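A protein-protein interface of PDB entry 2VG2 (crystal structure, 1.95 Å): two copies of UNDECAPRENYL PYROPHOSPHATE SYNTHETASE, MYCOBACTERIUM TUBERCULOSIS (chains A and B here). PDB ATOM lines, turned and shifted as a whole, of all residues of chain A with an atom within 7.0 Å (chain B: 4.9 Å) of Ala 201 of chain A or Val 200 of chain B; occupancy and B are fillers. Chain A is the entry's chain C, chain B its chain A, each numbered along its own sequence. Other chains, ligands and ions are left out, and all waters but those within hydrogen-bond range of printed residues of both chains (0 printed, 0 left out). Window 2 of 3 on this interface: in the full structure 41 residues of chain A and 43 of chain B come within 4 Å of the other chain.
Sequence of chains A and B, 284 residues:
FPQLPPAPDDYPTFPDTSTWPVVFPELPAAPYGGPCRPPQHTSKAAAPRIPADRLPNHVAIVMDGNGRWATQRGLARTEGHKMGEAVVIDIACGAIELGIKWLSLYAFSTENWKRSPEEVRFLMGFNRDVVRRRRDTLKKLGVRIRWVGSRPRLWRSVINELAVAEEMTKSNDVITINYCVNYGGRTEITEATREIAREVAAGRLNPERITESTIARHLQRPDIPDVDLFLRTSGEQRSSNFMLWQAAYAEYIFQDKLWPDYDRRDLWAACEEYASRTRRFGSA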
ATOM      1  N   THR A 193       8.948  22.145  -3.843  1.00  0.00           N
ATOM      2  CA  THR A 193       8.262  20.887  -3.589  1.00  0.00           C
ATOM      3  C   THR A 193       7.724  20.283  -4.872  1.00  0.00           C
ATOM      4  O   THR A 193       7.825  19.074  -5.062  1.00  0.00           O
ATOM      5  CB  THR A 193       7.129  21.070  -2.565  1.00  0.00           C
ATOM      6  OG1 THR A 193       7.698  21.511  -1.322  1.00  0.00           O
ATOM      7  CG2 THR A 193       6.378  19.761  -2.332  1.00  0.00           C
ATOM      8  N   ILE A 196      10.553  18.874  -6.867  1.00  0.00           N
ATOM      9  CA  ILE A 196      10.923  17.615  -6.219  1.00  0.00           C
ATOM     10  C   ILE A 196       9.943  16.488  -6.574  1.00  0.00           C
ATOM     11  O   ILE A 196      10.368  15.395  -6.934  1.00  0.00           O
ATOM     12  CB  ILE A 196      11.063  17.810  -4.687  1.00  0.00           C
ATOM     13  CG1 ILE A 196      12.337  18.633  -4.399  1.00  0.00           C
ATOM     14  CG2 ILE A 196      11.097  16.475  -3.965  1.00  0.00           C
ATOM     15  CD1 ILE A 196      12.411  19.193  -2.974  1.00  0.00           C
ATOM     16  N   ALA A 197       8.644  16.792  -6.507  1.00  0.00           N
ATOM     17  CA  ALA A 197       7.560  15.883  -6.902  1.00  0.00           C
ATOM     18  C   ALA A 197       7.659  15.391  -8.351  1.00  0.00           C
ATOM     19  O   ALA A 197       7.417  14.224  -8.612  1.00  0.00           O
ATOM     20  CB  ALA A 197       6.185  16.578  -6.686  1.00  0.00           C
ATOM     21  N   ARG A 198       7.976  16.280  -9.288  1.00  0.00           N
ATOM     22  CA  ARG A 198       8.227  15.879 -10.689  1.00  0.00           C
ATOM     23  C   ARG A 198       9.381  14.857 -10.811  1.00  0.00           C
ATOM     24  O   ARG A 198       9.280  13.857 -11.542  1.00  0.00           O
ATOM     25  CB  ARG A 198       8.549  17.118 -11.525  1.00  0.00           C
ATOM     26  CG  ARG A 198       7.350  18.009 -11.765  1.00  0.00           C
ATOM     27  CD  ARG A 198       7.754  19.258 -12.478  1.00  0.00           C
ATOM     28  NE  ARG A 198       6.640  20.194 -12.521  1.00  0.00           N
ATOM     29  CZ  ARG A 198       6.678  21.446 -12.089  1.00  0.00           C
ATOM     30  NH1 ARG A 198       7.794  21.977 -11.611  1.00  0.00           N
ATOM     31  NH2 ARG A 198       5.582  22.184 -12.171  1.00  0.00           N
ATOM     32  N   GLU A 199      10.464  15.104 -10.083  1.00  0.00           N
ATOM     33  CA  GLU A 199      11.616  14.193 -10.072  1.00  0.00           C
ATOM     34  C   GLU A 199      11.252  12.815  -9.498  1.00  0.00           C
ATOM     35  O   GLU A 199      11.663  11.775 -10.026  1.00  0.00           O
ATOM     36  CB  GLU A 199      12.776  14.813  -9.285  1.00  0.00           C
ATOM     37  CG  GLU A 199      13.392  16.031  -9.996  1.00  0.00           C
ATOM     38  CD  GLU A 199      13.993  15.656 -11.316  1.00  0.00           C
ATOM     39  OE1 GLU A 199      13.450  16.061 -12.363  1.00  0.00           O
ATOM     40  OE2 GLU A 199      14.987  14.912 -11.324  1.00  0.00           O
ATOM     41  N   VAL A 200      10.479  12.823  -8.420  1.00  0.00           N
ATOM     42  CA  VAL A 200       9.959  11.584  -7.831  1.00  0.00           C
ATOM     43  C   VAL A 200       9.042  10.847  -8.825  1.00  0.00           C
ATOM     44  O   VAL A 200       9.200   9.648  -9.046  1.00  0.00           O
ATOM     45  CB  VAL A 200       9.178  11.883  -6.542  1.00  0.00           C
ATOM     46  CG1 VAL A 200       8.442  10.629  -6.039  1.00  0.00           C
ATOM     47  CG2 VAL A 200      10.127  12.464  -5.458  1.00  0.00           C
ATOM     48  N   ALA A 201       8.113  11.577  -9.434  1.00  0.00           N
ATOM     49  CA  ALA A 201       7.224  11.008 -10.463  1.00  0.00           C
ATOM     50  C   ALA A 201       7.991  10.387 -11.663  1.00  0.00           C
ATOM     51  O   ALA A 201       7.567   9.368 -12.226  1.00  0.00           O
ATOM     52  CB  ALA A 201       6.250  12.072 -10.949  1.00  0.00           C
ATOM     53  N   ALA A 202       9.123  10.990 -12.032  1.00  0.00           N
ATOM     54  CA  ALA A 202       9.979  10.487 -13.128  1.00  0.00           C
ATOM     55  C   ALA A 202      10.939   9.341 -12.732  1.00  0.00           C
ATOM     56  O   ALA A 202      11.743   8.883 -13.557  1.00  0.00           O
ATOM     57  CB  ALA A 202      10.767  11.644 -13.734  1.00  0.00           C
ATOM     58  N   GLY A 203      10.853   8.876 -11.490  1.00  0.00           N
ATOM     59  CA  GLY A 203      11.697   7.778 -11.004  1.00  0.00           C
ATOM     60  C   GLY A 203      13.114   8.200 -10.622  1.00  0.00           C
ATOM     61  O   GLY A 203      13.946   7.354 -10.314  1.00  0.00           O
ATOM     62  N   ARG A 204      13.372   9.508 -10.601  1.00  0.00           N
ATOM     63  CA  ARG A 204      14.722  10.030 -10.407  1.00  0.00           C
ATOM     64  C   ARG A 204      15.066  10.431  -8.977  1.00  0.00           C
ATOM     65  O   ARG A 204      16.221  10.762  -8.691  1.00  0.00           O
ATOM     66  CB  ARG A 204      14.962  11.202 -11.365  1.00  0.00           C
ATOM     67  CG  ARG A 204      15.193  10.762 -12.794  1.00  0.00           C
ATOM     68  CD  ARG A 204      15.705  11.902 -13.661  1.00  0.00           C
ATOM     69  NE  ARG A 204      14.682  12.917 -13.790  1.00  0.00           N
ATOM     70  CZ  ARG A 204      13.790  12.998 -14.775  1.00  0.00           C
ATOM     71  NH1 ARG A 204      13.784  12.134 -15.781  1.00  0.00           N
ATOM     72  NH2 ARG A 204      12.894  13.968 -14.748  1.00  0.00           N
ATOM     73  N   LEU A 205      14.095  10.388  -8.065  1.00  0.00           N
ATOM     74  CA  LEU A 205      14.365  10.747  -6.676  1.00  0.00           C
ATOM     75  C   LEU A 205      13.570   9.868  -5.723  1.00  0.00           C
ATOM     76  O   LEU A 205      12.348   9.723  -5.856  1.00  0.00           O
ATOM     77  CB  LEU A 205      14.042  12.225  -6.444  1.00  0.00           C
ATOM     78  CG  LEU A 205      14.242  12.873  -5.065  1.00  0.00           C
ATOM     79  CD1 LEU A 205      15.677  12.723  -4.570  1.00  0.00           C
ATOM     80  CD2 LEU A 205      13.875  14.347  -5.171  1.00  0.00           C
ATOM     81  N   PRO A 207      11.838   9.381  -2.388  1.00  0.00           N
ATOM     82  CA  PRO A 207      11.283  10.240  -1.330  1.00  0.00           C
ATOM     83  C   PRO A 207      12.042  10.181   0.004  1.00  0.00           C
ATOM     84  O   PRO A 207      12.220  11.215   0.692  1.00  0.00           O
ATOM     85  CB  PRO A 207       9.855   9.701  -1.163  1.00  0.00           C
ATOM     86  CG  PRO A 207       9.497   9.186  -2.524  1.00  0.00           C
ATOM     87  CD  PRO A 207      10.784   8.593  -3.060  1.00  0.00           C
ATOM     88  N   ILE B 196       4.522  14.357   0.765  1.00  0.00           N
ATOM     89  CA  ILE B 196       4.012  14.676  -0.579  1.00  0.00           C
ATOM     90  C   ILE B 196       4.671  13.779  -1.632  1.00  0.00           C
ATOM     91  O   ILE B 196       3.988  13.172  -2.466  1.00  0.00           O
ATOM     92  CB  ILE B 196       4.180  16.168  -0.900  1.00  0.00           C
ATOM     93  CG1 ILE B 196       3.141  16.972  -0.101  1.00  0.00           C
ATOM     94  CG2 ILE B 196       4.045  16.439  -2.418  1.00  0.00           C
ATOM     95  CD1 ILE B 196       3.415  18.475  -0.032  1.00  0.00           C
ATOM     96  N   ALA B 197       5.994  13.687  -1.561  1.00  0.00           N
ATOM     97  CA  ALA B 197       6.787  12.793  -2.411  1.00  0.00           C
ATOM     98  C   ALA B 197       6.294  11.334  -2.374  1.00  0.00           C
ATOM     99  O   ALA B 197       6.181  10.684  -3.414  1.00  0.00           O
ATOM    100  CB  ALA B 197       8.262  12.863  -2.004  1.00  0.00           C
ATOM    101  N   ARG B 198       5.988  10.835  -1.179  1.00  0.00           N
ATOM    102  CA  ARG B 198       5.497   9.457  -1.011  1.00  0.00           C
ATOM    103  C   ARG B 198       4.157   9.297  -1.687  1.00  0.00           C
ATOM    104  O   ARG B 198       3.925   8.315  -2.371  1.00  0.00           O
ATOM    105  CB  ARG B 198       5.355   9.087   0.467  1.00  0.00           C
ATOM    106  CG  ARG B 198       6.671   8.991   1.188  1.00  0.00           C
ATOM    107  CD  ARG B 198       6.492   8.948   2.683  1.00  0.00           C
ATOM    108  NE  ARG B 198       7.802   8.875   3.333  1.00  0.00           N
ATOM    109  CZ  ARG B 198       8.191   9.603   4.374  1.00  0.00           C
ATOM    110  NH1 ARG B 198       7.378  10.453   4.958  1.00  0.00           N
ATOM    111  NH2 ARG B 198       9.418   9.453   4.854  1.00  0.00           N
ATOM    112  N   GLU B 199       3.289  10.283  -1.501  1.00  0.00           N
ATOM    113  CA  GLU B 199       1.978  10.294  -2.157  1.00  0.00           C
ATOM    114  C   GLU B 199       2.086  10.302  -3.685  1.00  0.00           C
ATOM    115  O   GLU B 199       1.371   9.566  -4.389  1.00  0.00           O
ATOM    116  CB  GLU B 199       1.161  11.489  -1.675  1.00  0.00           C
ATOM    117  CG  GLU B 199       0.714  11.405  -0.232  1.00  0.00           C
ATOM    118  CD  GLU B 199      -0.152  10.190   0.030  1.00  0.00           C
ATOM    119  OE1 GLU B 199       0.291   9.306   0.800  1.00  0.00           O
ATOM    120  OE2 GLU B 199      -1.257  10.103  -0.561  1.00  0.00           O
ATOM    121  N   VAL B 200       2.981  11.132  -4.201  1.00  0.00           N
ATOM    122  CA  VAL B 200       3.266  11.138  -5.628  1.00  0.00           C
ATOM    123  C   VAL B 200       3.809   9.797  -6.116  1.00  0.00           C
ATOM    124  O   VAL B 200       3.385   9.304  -7.157  1.00  0.00           O
ATOM    125  CB  VAL B 200       4.268  12.257  -6.007  1.00  0.00           C
ATOM    126  CG1 VAL B 200       4.731  12.089  -7.464  1.00  0.00           C
ATOM    127  CG2 VAL B 200       3.624  13.630  -5.785  1.00  0.00           C
ATOM    128  N   ALA B 201       4.744   9.210  -5.374  1.00  0.00           N
ATOM    129  CA  ALA B 201       5.319   7.908  -5.747  1.00  0.00           C
ATOM    130  C   ALA B 201       4.236   6.828  -5.846  1.00  0.00           C
ATOM    131  O   ALA B 201       4.317   5.936  -6.691  1.00  0.00           O
ATOM    132  CB  ALA B 201       6.384   7.487  -4.744  1.00  0.00           C
ATOM    133  N   ALA B 202       3.236   6.927  -4.968  1.00  0.00           N
ATOM    134  CA  ALA B 202       2.100   6.004  -4.929  1.00  0.00           C
ATOM    135  C   ALA B 202       1.007   6.364  -5.947  1.00  0.00           C
ATOM    136  O   ALA B 202       0.007   5.653  -6.059  1.00  0.00           O
ATOM    137  CB  ALA B 202       1.511   5.968  -3.523  1.00  0.00           C
ATOM    138  N   GLY B 203       1.190   7.454  -6.684  1.00  0.00           N
ATOM    139  CA  GLY B 203       0.238   7.872  -7.723  1.00  0.00           C
ATOM    140  C   GLY B 203      -1.001   8.634  -7.244  1.00  0.00           C
ATOM    141  O   GLY B 203      -1.861   8.995  -8.068  1.00  0.00           O
ATOM    142  N   ARG B 204      -1.075   8.879  -5.938  1.00  0.00           N
ATOM    143  CA  ARG B 204      -2.234   9.501  -5.278  1.00  0.00           C
ATOM    144  C   ARG B 204      -2.207  11.022  -5.311  1.00  0.00           C
ATOM    145  O   ARG B 204      -3.097  11.675  -4.745  1.00  0.00           O
ATOM    146  CB  ARG B 204      -2.311   9.054  -3.818  1.00  0.00           C
ATOM    147  CG  ARG B 204      -2.538   7.553  -3.646  1.00  0.00           C
ATOM    148  CD  ARG B 204      -2.889   7.193  -2.215  1.00  0.00           C
ATOM    149  NE  ARG B 204      -1.731   7.261  -1.331  1.00  0.00           N
ATOM    150  CZ  ARG B 204      -0.895   6.252  -1.073  1.00  0.00           C
ATOM    151  NH1 ARG B 204      -1.075   5.056  -1.613  1.00  0.00           N
ATOM    152  NH2 ARG B 204       0.136   6.448  -0.249  1.00  0.00           N
ATOM    153  N   LEU B 205      -1.183  11.583  -5.950  1.00  0.00           N
ATOM    154  CA  LEU B 205      -1.049  13.017  -6.091  1.00  0.00           C
ATOM    155  C   LEU B 205      -0.307  13.304  -7.392  1.00  0.00           C
ATOM    156  O   LEU B 205       0.767  12.750  -7.636  1.00  0.00           O
ATOM    157  CB  LEU B 205      -0.299  13.561  -4.868  1.00  0.00           C
ATOM    158  CG  LEU B 205      -0.141  15.061  -4.645  1.00  0.00           C
ATOM    159  CD1 LEU B 205      -1.490  15.800  -4.695  1.00  0.00           C
ATOM    160  CD2 LEU B 205       0.558  15.264  -3.286  1.00  0.00           C
ATOM    161  N   PRO B 207       1.865  15.805  -9.398  1.00  0.00           N
ATOM    162  CA  PRO B 207       2.768  16.915  -9.063  1.00  0.00           C
ATOM    163  C   PRO B 207       2.293  18.282  -9.532  1.00  0.00           C
ATOM    164  O   PRO B 207       2.589  19.287  -8.885  1.00  0.00           O
ATOM    165  CB  PRO B 207       4.055  16.542  -9.799  1.00  0.00           C
ATOM    166  CG  PRO B 207       4.044  15.078  -9.820  1.00  0.00           C
ATOM    167  CD  PRO B 207       2.601  14.736 -10.098  1.00  0.00           C
ATOM    168  N   ILE B 210      -0.002  20.269  -6.999  1.00  0.00           N
ATOM    169  CA  ILE B 210       0.494  20.671  -5.691  1.00  0.00           C
ATOM    170  C   ILE B 210       0.377  22.191  -5.575  1.00  0.00           C
ATOM    171  O   ILE B 210       0.845  22.910  -6.450  1.00  0.00           O
ATOM    172  CB  ILE B 210       1.952  20.255  -5.494  1.00  0.00           C
ATOM    173  CG1 ILE B 210       2.077  18.726  -5.468  1.00  0.00           C
ATOM    174  CG2 ILE B 210       2.526  20.872  -4.204  1.00  0.00           C
ATOM    175  CD1 ILE B 210       3.509  18.219  -5.580  1.00  0.00           C
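Among the printed residues, pairs that only touch across the chains: Thr 193 of chain A with Ile 196 of chain B (3.97 Å), Ala 197 of chain A with Val 200 of chain B (3.6 Å), Ala 197 of chain A with Pro 207 of chain B (3.7 Å), Ala 197 of chain A with Ile 210 of chain B (3.3 Å), Arg 198 of chain A with Pro 207 of chain B (3.96 Å), Val 200 of chain A with Ala 197 of chain B (3.5 Å), Val 200 of chain A with Ala 201 of chain B (3.97 Å), Ala 201 of chain A with Val 200 of chain B (3.8 Å), Ala 201 of chain A with Pro 207 of chain B (3.9 Å) and Pro 207 of chain A with Ala 197 of chain B (3.6 Å).
Printed residues of chain A that touch a printed residue of chain B: Thr 193, Ala 197, Arg 198, Val 200, Ala 201 and Pro 207. Hydrophobic or aromatic side chains of chain A that line the printed part of chain B: Ala 197, Val 200, Ala 201 and Pro 207. Of the 12 printed residues of chain B, 6 touch a printed residue of chain A.
Of chain B, only Val 200 (3.8 Å) and Pro 207 (3.9 Å) come within 4 Å of Ala 201 of chain A. Of chain A, only Ala 197 (3.6 Å) and Ala 201 (3.8 Å) come within 4 Å of Val 200 of chain B. Of the printed residues of chain B, Ala 197 of chain A touches Val 200, Pro 207 and Ile 210. Of the printed residues of chain A, Ile 210 of chain B touches Ala 197 (3.3 Å). Of the printed residues of chain B, Pro 207 of chain A touches Ala 197. Printed residues of chain A within 4 Å of Pro 207 of chain B: Ala 197 (3.7 Å), Arg 198 (3.96 Å) and Ala 201 (3.9 Å). Of the printed residues of chain A, Ala 201 of chain B touches Val 200 (3.97 Å).
Ala 197 of chain A touches Val 200 of chain B, and with the chains exchanged Val 200 of chain A touches Ala 197 of chain B. Arg 198 of chain A touches Pro 207 of chain B, but with the chains exchanged Pro 207 of chain A does not touch Arg 198 of chain B (4.02 Å). Val 200 of chain A touches Ala 201 of chain B, and with the chains exchanged Ala 201 of chain A touches Val 200 of chain B. Ala 201 of chain A touches Pro 207 of chain B, but with the chains exchanged Pro 207 of chain A does not touch Ala 201 of chain B (4.2 Å). Positions printed for both chains: 196, 197, 198, 199, 200, 201, 202, 203, 204, 205 and 207. Of the 10 pairs that touch across the chains among the printed residues, 6 have their exchanged pair printed and touching as well.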
